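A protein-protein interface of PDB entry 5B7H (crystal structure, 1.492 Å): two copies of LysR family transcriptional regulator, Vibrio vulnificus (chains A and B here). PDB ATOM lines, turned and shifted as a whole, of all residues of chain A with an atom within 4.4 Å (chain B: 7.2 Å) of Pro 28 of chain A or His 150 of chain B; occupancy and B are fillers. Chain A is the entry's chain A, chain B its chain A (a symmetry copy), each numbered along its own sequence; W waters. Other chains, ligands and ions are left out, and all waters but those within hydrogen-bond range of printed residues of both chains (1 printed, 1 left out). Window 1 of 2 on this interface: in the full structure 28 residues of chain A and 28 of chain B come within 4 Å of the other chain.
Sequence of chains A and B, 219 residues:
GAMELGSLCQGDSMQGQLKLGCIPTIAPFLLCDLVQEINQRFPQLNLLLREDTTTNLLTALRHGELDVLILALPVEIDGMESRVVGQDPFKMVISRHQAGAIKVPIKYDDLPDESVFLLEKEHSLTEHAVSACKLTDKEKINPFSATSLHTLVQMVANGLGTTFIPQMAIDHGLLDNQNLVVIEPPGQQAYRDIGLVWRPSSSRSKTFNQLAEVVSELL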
ATOM      1  N   PRO A  24      -4.085  -6.630 -13.182  1.00  0.00           N
ATOM      2  CA  PRO A  24      -4.918  -7.489 -14.035  1.00  0.00           C
ATOM      3  C   PRO A  24      -5.918  -8.375 -13.299  1.00  0.00           C
ATOM      4  O   PRO A  24      -6.912  -8.740 -13.922  1.00  0.00           O
ATOM      5  CB  PRO A  24      -3.888  -8.345 -14.788  1.00  0.00           C
ATOM      6  CG  PRO A  24      -2.675  -7.494 -14.807  1.00  0.00           C
ATOM      7  CD  PRO A  24      -2.652  -6.808 -13.459  1.00  0.00           C
ATOM      8  N   ILE A  26      -7.716  -7.501 -10.723  1.00  0.00           N
ATOM      9  CA  ILE A  26      -8.783  -6.661 -10.195  1.00  0.00           C
ATOM     10  C   ILE A  26      -9.513  -5.947 -11.322  1.00  0.00           C
ATOM     11  O   ILE A  26     -10.749  -5.918 -11.346  1.00  0.00           O
ATOM     12  CB  ILE A  26      -8.246  -5.629  -9.168  1.00  0.00           C
ATOM     13  CG1 ILE A  26      -7.616  -6.328  -7.952  1.00  0.00           C
ATOM     14  CG2 ILE A  26      -9.386  -4.688  -8.747  1.00  0.00           C
ATOM     15  CD1 ILE A  26      -6.979  -5.312  -6.984  1.00  0.00           C
ATOM     16  N   ALA A  27      -8.761  -5.401 -12.285  1.00  0.00           N
ATOM     17  CA  ALA A  27      -9.325  -4.473 -13.276  1.00  0.00           C
ATOM     18  C   ALA A  27     -10.552  -4.996 -14.019  1.00  0.00           C
ATOM     19  O   ALA A  27     -11.535  -4.236 -14.124  1.00  0.00           O
ATOM     20  CB  ALA A  27      -8.240  -4.033 -14.266  1.00  0.00           C
ATOM     21  N   PRO A  28     -10.574  -6.234 -14.529  1.00  0.00           N
ATOM     22  CA  PRO A  28     -11.738  -6.679 -15.320  1.00  0.00           C
ATOM     23  C   PRO A  28     -12.994  -6.788 -14.485  1.00  0.00           C
ATOM     24  O   PRO A  28     -14.065  -6.919 -15.070  1.00  0.00           O
ATOM     25  CB  PRO A  28     -11.333  -8.068 -15.820  1.00  0.00           C
ATOM     26  CG  PRO A  28      -9.853  -8.145 -15.648  1.00  0.00           C
ATOM     27  CD  PRO A  28      -9.536  -7.278 -14.441  1.00  0.00           C
ATOM     28  N   PHE A  29     -12.880  -6.851 -13.153  1.00  0.00           N
ATOM     29  CA  PHE A  29     -14.022  -7.169 -12.300  1.00  0.00           C
ATOM     30  C   PHE A  29     -14.491  -5.890 -11.614  1.00  0.00           C
ATOM     31  O   PHE A  29     -15.509  -5.304 -12.008  1.00  0.00           O
ATOM     32  CB  PHE A  29     -13.578  -8.270 -11.333  1.00  0.00           C
ATOM     33  CG  PHE A  29     -12.766  -9.384 -12.024  1.00  0.00           C
ATOM     34  CD1 PHE A  29     -13.333 -10.144 -13.062  1.00  0.00           C
ATOM     35  CD2 PHE A  29     -11.451  -9.610 -11.669  1.00  0.00           C
ATOM     36  CE1 PHE A  29     -12.604 -11.145 -13.704  1.00  0.00           C
ATOM     37  CE2 PHE A  29     -10.711 -10.597 -12.300  1.00  0.00           C
ATOM     38  CZ  PHE A  29     -11.285 -11.366 -13.333  1.00  0.00           C
ATOM     39  N   LEU A  30     -13.708  -5.366 -10.678  1.00  0.00           N
ATOM     40  CA  LEU A  30     -14.151  -4.252  -9.854  1.00  0.00           C
ATOM     41  C   LEU A  30     -14.393  -2.981 -10.651  1.00  0.00           C
ATOM     42  O   LEU A  30     -15.281  -2.187 -10.296  1.00  0.00           O
ATOM     43  CB  LEU A  30     -13.085  -4.000  -8.784  1.00  0.00           C
ATOM     44  CG  LEU A  30     -13.213  -2.785  -7.888  1.00  0.00           C
ATOM     45  CD1 LEU A  30     -14.436  -2.924  -6.982  1.00  0.00           C
ATOM     46  CD2 LEU A  30     -11.921  -2.649  -7.021  1.00  0.00           C
ATOM     47  N   CYS A  32     -15.641  -2.437 -13.574  1.00  0.00           N
ATOM     48  CA  CYS A  32     -16.943  -2.369 -14.217  1.00  0.00           C
ATOM     49  C   CYS A  32     -17.940  -1.753 -13.248  1.00  0.00           C
ATOM     50  O   CYS A  32     -18.711  -0.845 -13.606  1.00  0.00           O
ATOM     51  CB  CYS A  32     -17.417  -3.789 -14.572  1.00  0.00           C
ATOM     52  SG  CYS A  32     -16.462  -4.628 -15.863  1.00  0.00           S
ATOM     53  N   HIS A 150      -7.444 -15.683 -16.809  1.00  0.00           N
ATOM     54  CA  HIS A 150      -8.374 -16.441 -17.656  1.00  0.00           C
ATOM     55  C   HIS A 150      -7.762 -17.744 -18.111  1.00  0.00           C
ATOM     56  O   HIS A 150      -8.441 -18.785 -18.132  1.00  0.00           O
ATOM     57  CB  HIS A 150      -8.715 -15.626 -18.895  1.00  0.00           C
ATOM     58  CG  HIS A 150      -9.277 -14.299 -18.559  1.00  0.00           C
ATOM     59  ND1 HIS A 150      -8.475 -13.197 -18.321  1.00  0.00           N
ATOM     60  CD2 HIS A 150     -10.555 -13.907 -18.347  1.00  0.00           C
ATOM     61  CE1 HIS A 150      -9.249 -12.170 -17.999  1.00  0.00           C
ATOM     62  NE2 HIS A 150     -10.513 -12.576 -18.002  1.00  0.00           N
ATOM     63  N   PRO B  24      -4.094 -11.663 -25.995  1.00  0.00           N
ATOM     64  CA  PRO B  24      -5.058 -11.243 -24.969  1.00  0.00           C
ATOM     65  C   PRO B  24      -6.467 -10.947 -25.472  1.00  0.00           C
ATOM     66  O   PRO B  24      -7.386 -11.049 -24.663  1.00  0.00           O
ATOM     67  CB  PRO B  24      -4.417  -9.979 -24.378  1.00  0.00           C
ATOM     68  CG  PRO B  24      -2.968 -10.179 -24.616  1.00  0.00           C
ATOM     69  CD  PRO B  24      -2.877 -10.838 -25.975  1.00  0.00           C
ATOM     70  N   PRO B  28      -9.320 -14.922 -23.515  1.00  0.00           N
ATOM     71  CA  PRO B  28     -10.394 -15.024 -22.508  1.00  0.00           C
ATOM     72  C   PRO B  28     -11.688 -15.539 -23.097  1.00  0.00           C
ATOM     73  O   PRO B  28     -12.575 -15.886 -22.322  1.00  0.00           O
ATOM     74  CB  PRO B  28     -10.586 -13.583 -22.029  1.00  0.00           C
ATOM     75  CG  PRO B  28      -9.363 -12.846 -22.462  1.00  0.00           C
ATOM     76  CD  PRO B  28      -8.909 -13.524 -23.744  1.00  0.00           C
ATOM     77  N   PHE B  29     -11.859 -15.489 -24.423  1.00  0.00           N
ATOM     78  CA  PHE B  29     -13.152 -15.767 -25.040  1.00  0.00           C
ATOM     79  C   PHE B  29     -13.101 -17.148 -25.686  1.00  0.00           C
ATOM     80  O   PHE B  29     -13.648 -18.116 -25.140  1.00  0.00           O
ATOM     81  CB  PHE B  29     -13.445 -14.629 -26.022  1.00  0.00           C
ATOM     82  CG  PHE B  29     -13.122 -13.238 -25.441  1.00  0.00           C
ATOM     83  CD1 PHE B  29     -13.775 -12.776 -24.284  1.00  0.00           C
ATOM     84  CD2 PHE B  29     -12.144 -12.451 -26.017  1.00  0.00           C
ATOM     85  CE1 PHE B  29     -13.481 -11.525 -23.741  1.00  0.00           C
ATOM     86  CE2 PHE B  29     -11.837 -11.208 -25.487  1.00  0.00           C
ATOM     87  CZ  PHE B  29     -12.502 -10.742 -24.335  1.00  0.00           C
ATOM     88  N   GLU B  51      -0.684 -16.813 -22.339  1.00  0.00           N
ATOM     89  CA  GLU B  51      -1.258 -15.611 -22.913  1.00  0.00           C
ATOM     90  C   GLU B  51      -0.156 -14.562 -22.996  1.00  0.00           C
ATOM     91  O   GLU B  51       0.529 -14.275 -21.998  1.00  0.00           O
ATOM     92  CB  GLU B  51      -2.436 -15.122 -22.054  1.00  0.00           C
ATOM     93  CG  GLU B  51      -3.050 -13.855 -22.623  1.00  0.00           C
ATOM     94  CD  GLU B  51      -4.293 -13.387 -21.852  1.00  0.00           C
ATOM     95  OE1 GLU B  51      -4.389 -12.146 -21.646  1.00  0.00           O
ATOM     96  OE2 GLU B  51      -5.118 -14.214 -21.442  1.00  0.00           O
ATOM     97  N   LEU B 119      -6.330   0.394 -28.108  1.00  0.00           N
ATOM     98  CA  LEU B 119      -5.186  -0.184 -27.420  1.00  0.00           C
ATOM     99  C   LEU B 119      -3.869   0.319 -28.017  1.00  0.00           C
ATOM    100  O   LEU B 119      -3.772   0.668 -29.212  1.00  0.00           O
ATOM    101  CB  LEU B 119      -5.187  -1.713 -27.548  1.00  0.00           C
ATOM    102  CG  LEU B 119      -6.388  -2.382 -26.889  1.00  0.00           C
ATOM    103  CD1 LEU B 119      -6.489  -3.846 -27.345  1.00  0.00           C
ATOM    104  CD2 LEU B 119      -6.298  -2.338 -25.314  1.00  0.00           C
ATOM    105  N   THR B 147      -4.590  -0.158 -22.352  1.00  0.00           N
ATOM    106  CA  THR B 147      -3.647  -1.252 -22.168  1.00  0.00           C
ATOM    107  C   THR B 147      -4.314  -2.614 -21.958  1.00  0.00           C
ATOM    108  O   THR B 147      -3.605  -3.613 -21.839  1.00  0.00           O
ATOM    109  CB  THR B 147      -2.697  -0.890 -21.022  1.00  0.00           C
ATOM    110  OG1 THR B 147      -3.503  -0.281 -19.997  1.00  0.00           O
ATOM    111  CG2 THR B 147      -1.751   0.181 -21.511  1.00  0.00           C
ATOM    112  N   SER B 148      -5.639  -2.694 -21.952  1.00  0.00           N
ATOM    113  CA  SER B 148      -6.316  -3.994 -21.959  1.00  0.00           C
ATOM    114  C   SER B 148      -7.706  -3.787 -22.555  1.00  0.00           C
ATOM    115  O   SER B 148      -8.284  -2.682 -22.488  1.00  0.00           O
ATOM    116  CB  SER B 148      -6.428  -4.589 -20.535  1.00  0.00           C
ATOM    117  OG  SER B 148      -7.400  -3.904 -19.751  1.00  0.00           O
ATOM    118  N   LEU B 149      -8.256  -4.858 -23.145  1.00  0.00           N
ATOM    119  CA  LEU B 149      -9.575  -4.702 -23.720  1.00  0.00           C
ATOM    120  C   LEU B 149     -10.623  -4.405 -22.630  1.00  0.00           C
ATOM    121  O   LEU B 149     -11.557  -3.630 -22.892  1.00  0.00           O
ATOM    122  CB  LEU B 149      -9.910  -5.999 -24.466  1.00  0.00           C
ATOM    123  CG  LEU B 149     -11.236  -6.015 -25.263  1.00  0.00           C
ATOM    124  CD1 LEU B 149     -11.294  -4.920 -26.280  1.00  0.00           C
ATOM    125  CD2 LEU B 149     -11.459  -7.383 -25.960  1.00  0.00           C
ATOM    126  N   HIS B 150     -10.502  -4.997 -21.424  1.00  0.00           N
ATOM    127  CA  HIS B 150     -11.505  -4.712 -20.390  1.00  0.00           C
ATOM    128  C   HIS B 150     -11.485  -3.255 -19.996  1.00  0.00           C
ATOM    129  O   HIS B 150     -12.549  -2.640 -19.806  1.00  0.00           O
ATOM    130  CB  HIS B 150     -11.205  -5.537 -19.147  1.00  0.00           C
ATOM    131  CG  HIS B 150     -11.149  -6.987 -19.434  1.00  0.00           C
ATOM    132  ND1 HIS B 150      -9.989  -7.610 -19.862  1.00  0.00           N
ATOM    133  CD2 HIS B 150     -12.120  -7.929 -19.429  1.00  0.00           C
ATOM    134  CE1 HIS B 150     -10.252  -8.890 -20.084  1.00  0.00           C
ATOM    135  NE2 HIS B 150     -11.537  -9.108 -19.834  1.00  0.00           N
ATOM    136  N   THR B 151     -10.291  -2.686 -19.841  1.00  0.00           N
ATOM    137  CA  THR B 151     -10.245  -1.285 -19.390  1.00  0.00           C
ATOM    138  C   THR B 151     -10.616  -0.327 -20.519  1.00  0.00           C
ATOM    139  O   THR B 151     -11.199   0.739 -20.267  1.00  0.00           O
ATOM    140  CB  THR B 151      -8.911  -0.924 -18.733  1.00  0.00           C
ATOM    141  OG1 THR B 151      -7.832  -1.177 -19.647  1.00  0.00           O
ATOM    142  CG2 THR B 151      -8.699  -1.673 -17.415  1.00  0.00           C
ATOM    143  N   LEU B 152     -10.345  -0.715 -21.763  1.00  0.00           N
ATOM    144  CA  LEU B 152     -10.840   0.050 -22.898  1.00  0.00           C
ATOM    145  C   LEU B 152     -12.362   0.137 -22.876  1.00  0.00           C
ATOM    146  O   LEU B 152     -12.955   1.233 -23.016  1.00  0.00           O
ATOM    147  CB  LEU B 152     -10.358  -0.626 -24.179  1.00  0.00           C
ATOM    148  CG  LEU B 152     -10.825  -0.072 -25.522  1.00  0.00           C
ATOM    149  CD1 LEU B 152     -10.450   1.381 -25.654  1.00  0.00           C
ATOM    150  CD2 LEU B 152     -10.186  -0.950 -26.631  1.00  0.00           C
ATOM    151  N   VAL B 153     -13.025  -1.010 -22.716  1.00  0.00           N
ATOM    152  CA  VAL B 153     -14.481  -1.021 -22.706  1.00  0.00           C
ATOM    153  C   VAL B 153     -15.021  -0.250 -21.506  1.00  0.00           C
ATOM    154  O   VAL B 153     -16.047   0.454 -21.611  1.00  0.00           O
ATOM    155  CB  VAL B 153     -14.943  -2.484 -22.700  1.00  0.00           C
ATOM    156  CG1 VAL B 153     -16.450  -2.549 -22.312  1.00  0.00           C
ATOM    157  CG2 VAL B 153     -14.651  -3.093 -24.097  1.00  0.00           C
ATOM    158  N   GLN B 154     -14.333  -0.326 -20.357  1.00  0.00           N
ATOM    159  CA  GLN B 154     -14.775   0.441 -19.194  1.00  0.00           C
ATOM    160  C   GLN B 154     -14.697   1.945 -19.451  1.00  0.00           C
ATOM    161  O   GLN B 154     -15.575   2.689 -19.008  1.00  0.00           O
ATOM    162  CB  GLN B 154     -13.958   0.081 -17.955  1.00  0.00           C
ATOM    163  CG  GLN B 154     -14.267  -1.344 -17.448  1.00  0.00           C
ATOM    164  CD  GLN B 154     -13.112  -2.000 -16.711  1.00  0.00           C
ATOM    165  OE1 GLN B 154     -12.003  -1.434 -16.619  1.00  0.00           O
ATOM    166  NE2 GLN B 154     -13.338  -3.222 -16.268  1.00  0.00           N
ATOM    167  N   MET B 155     -13.666   2.424 -20.146  1.00  0.00           N
ATOM    168  CA  MET B 155     -13.632   3.855 -20.483  1.00  0.00           C
ATOM    169  C   MET B 155     -14.786   4.242 -21.402  1.00  0.00           C
ATOM    170  O   MET B 155     -15.391   5.312 -21.234  1.00  0.00           O
ATOM    171  CB  MET B 155     -12.307   4.266 -21.120  1.00  0.00           C
ATOM    172  CG  MET B 155     -11.164   4.241 -20.117  1.00  0.00           C
ATOM    173  SD  MET B 155      -9.621   4.895 -20.754  1.00  0.00           S
ATOM    174  CE  MET B 155      -9.083   3.569 -21.836  1.00  0.00           C
ATOM    175  N   VAL B 156     -15.132   3.373 -22.361  1.00  0.00           N
ATOM    176  CA  VAL B 156     -16.299   3.648 -23.197  1.00  0.00           C
ATOM    177  C   VAL B 156     -17.548   3.650 -22.332  1.00  0.00           C
ATOM    178  O   VAL B 156     -18.432   4.506 -22.491  1.00  0.00           O
ATOM    179  CB  VAL B 156     -16.361   2.616 -24.343  1.00  0.00           C
ATOM    180  CG1 VAL B 156     -17.700   2.750 -25.119  1.00  0.00           C
ATOM    181  CG2 VAL B 156     -15.181   2.838 -25.312  1.00  0.00           C
ATOM    182  N   LEU B 174     -18.604  -9.692 -22.453  1.00  0.00           N
ATOM    183  CA  LEU B 174     -17.729  -8.609 -22.001  1.00  0.00           C
ATOM    184  C   LEU B 174     -18.548  -7.356 -21.690  1.00  0.00           C
ATOM    185  O   LEU B 174     -18.159  -6.566 -20.788  1.00  0.00           O
ATOM    186  CB  LEU B 174     -16.677  -8.315 -23.087  1.00  0.00           C
ATOM    187  CG  LEU B 174     -15.642  -7.246 -22.669  1.00  0.00           C
ATOM    188  CD1 LEU B 174     -14.740  -7.769 -21.553  1.00  0.00           C
ATOM    189  CD2 LEU B 174     -14.828  -6.902 -23.920  1.00  0.00           C
ATOM    190  N   GLN B 178     -22.738  -3.205 -18.345  1.00  0.00           N
ATOM    191  CA  GLN B 178     -22.029  -1.937 -18.548  1.00  0.00           C
ATOM    192  C   GLN B 178     -22.827  -0.921 -19.326  1.00  0.00           C
ATOM    193  O   GLN B 178     -22.307   0.153 -19.623  1.00  0.00           O
ATOM    194  CB  GLN B 178     -20.671  -2.183 -19.232  1.00  0.00           C
ATOM    195  CG  GLN B 178     -19.832  -3.178 -18.406  1.00  0.00           C
ATOM    196  CD  GLN B 178     -18.356  -2.999 -18.668  1.00  0.00           C
ATOM    197  OE1 GLN B 178     -17.798  -1.990 -18.271  1.00  0.00           O
ATOM    198  NE2 GLN B 178     -17.729  -3.966 -19.362  1.00  0.00           N
HETATM  199  O   HOH W   1     -18.981  -0.301 -16.425  1.00  0.00           O
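The backbone carbonyl oxygen (O) of Ala 27 of chain A lies within hydrogen-bond range of the side-chain amide nitrogen (NE2) of Gln 154 of chain B (3.0 Å).
SG of Cys 32 of chain A sits at hydrogen-bond distance from NE2 of Gln 154 of chain B (3.4 Å).
SG of Cys 32 of chain A sits close to NE2 of Gln 178 of chain B.
The side-chain sulfur (SG) of Cys 32 of chain A sits at hydrogen-bond distance from the backbone carbonyl oxygen (O) of Pro 28 of chain A (3.4 Å).
The side-chain hydroxyl of Thr 151 of chain B lies within hydrogen-bond range of the side-chain hydroxyl of Ser 148 of chain B (2.8 Å).
The backbone carbonyl oxygen of His 150 of chain B sits close to the side-chain amide oxygen of Gln 154 of chain B (3.5 Å).
The side-chain amide nitrogen of Gln 178 of chain B is in hydrogen-bond range of the backbone carbonyl oxygen of Leu 174 of chain B (3.0 Å).
Among the printed residues, merely in contact across the chains: Ala 27 of chain A with Thr 151 of chain B, Pro 28 of chain A with His 150 of chain B, Pro 28 of chain A with Gln 154 of chain B and His 150 of chain A with Pro 28 of chain B.
Phe 29 of chain A touches none of the printed residues of chain B.
Of the printed residues of chain B, Cys 32 of chain A touches Gln 154 and Gln 178.
Printed residues of chain B within 4 Å of His 150 of chain A: Pro 28 (3.7 Å).
Of the printed residues of chain A, Thr 151 of chain B touches Ala 27.
Of the printed residues of chain A, Gln 154 of chain B touches Ala 27 (3.0 Å), Pro 28 (3.9 Å) and Cys 32 (3.4 Å).
Printed residues of chain A within 4 Å of Gln 178 of chain B: Cys 32.
The nearest residue of chain B that does not touch Pro 28 of chain A is Thr 151 of chain B (5.7 Å).
The nearest printed residue of chain A that does not touch His 150 of chain B is His 150 of chain A (4.01 Å).
The nearest printed residue of chain A that does not touch Pro 28 of chain B is Pro 28 of chain A (8.3 Å).
Hydrophobic or aromatic side chains of chain B that line the printed part of chain A: Pro 28 and His 150.
Hydrophobic or aromatic side chains of chain A within 4 Å of the printed part of chain B: Ala 27, Pro 28 and His 150.
Among the printed residues, no Asp or Glu carboxylate lies within 4 Å of a Lys or Arg side-chain nitrogen of the other chain.
Pro 28 of chain A touches His 150 of chain B, and with the chains exchanged His 150 of chain A touches Pro 28 of chain B.
Positions printed for both chains: 24, 28, 29 and 150.
Water W1 bridges the side-chain amide oxygen (OE1) of Gln 178 of chain B (2.8 Å) and the backbone carbonyl oxygen (O) of Cys 32 of chain A (2.9 Å).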
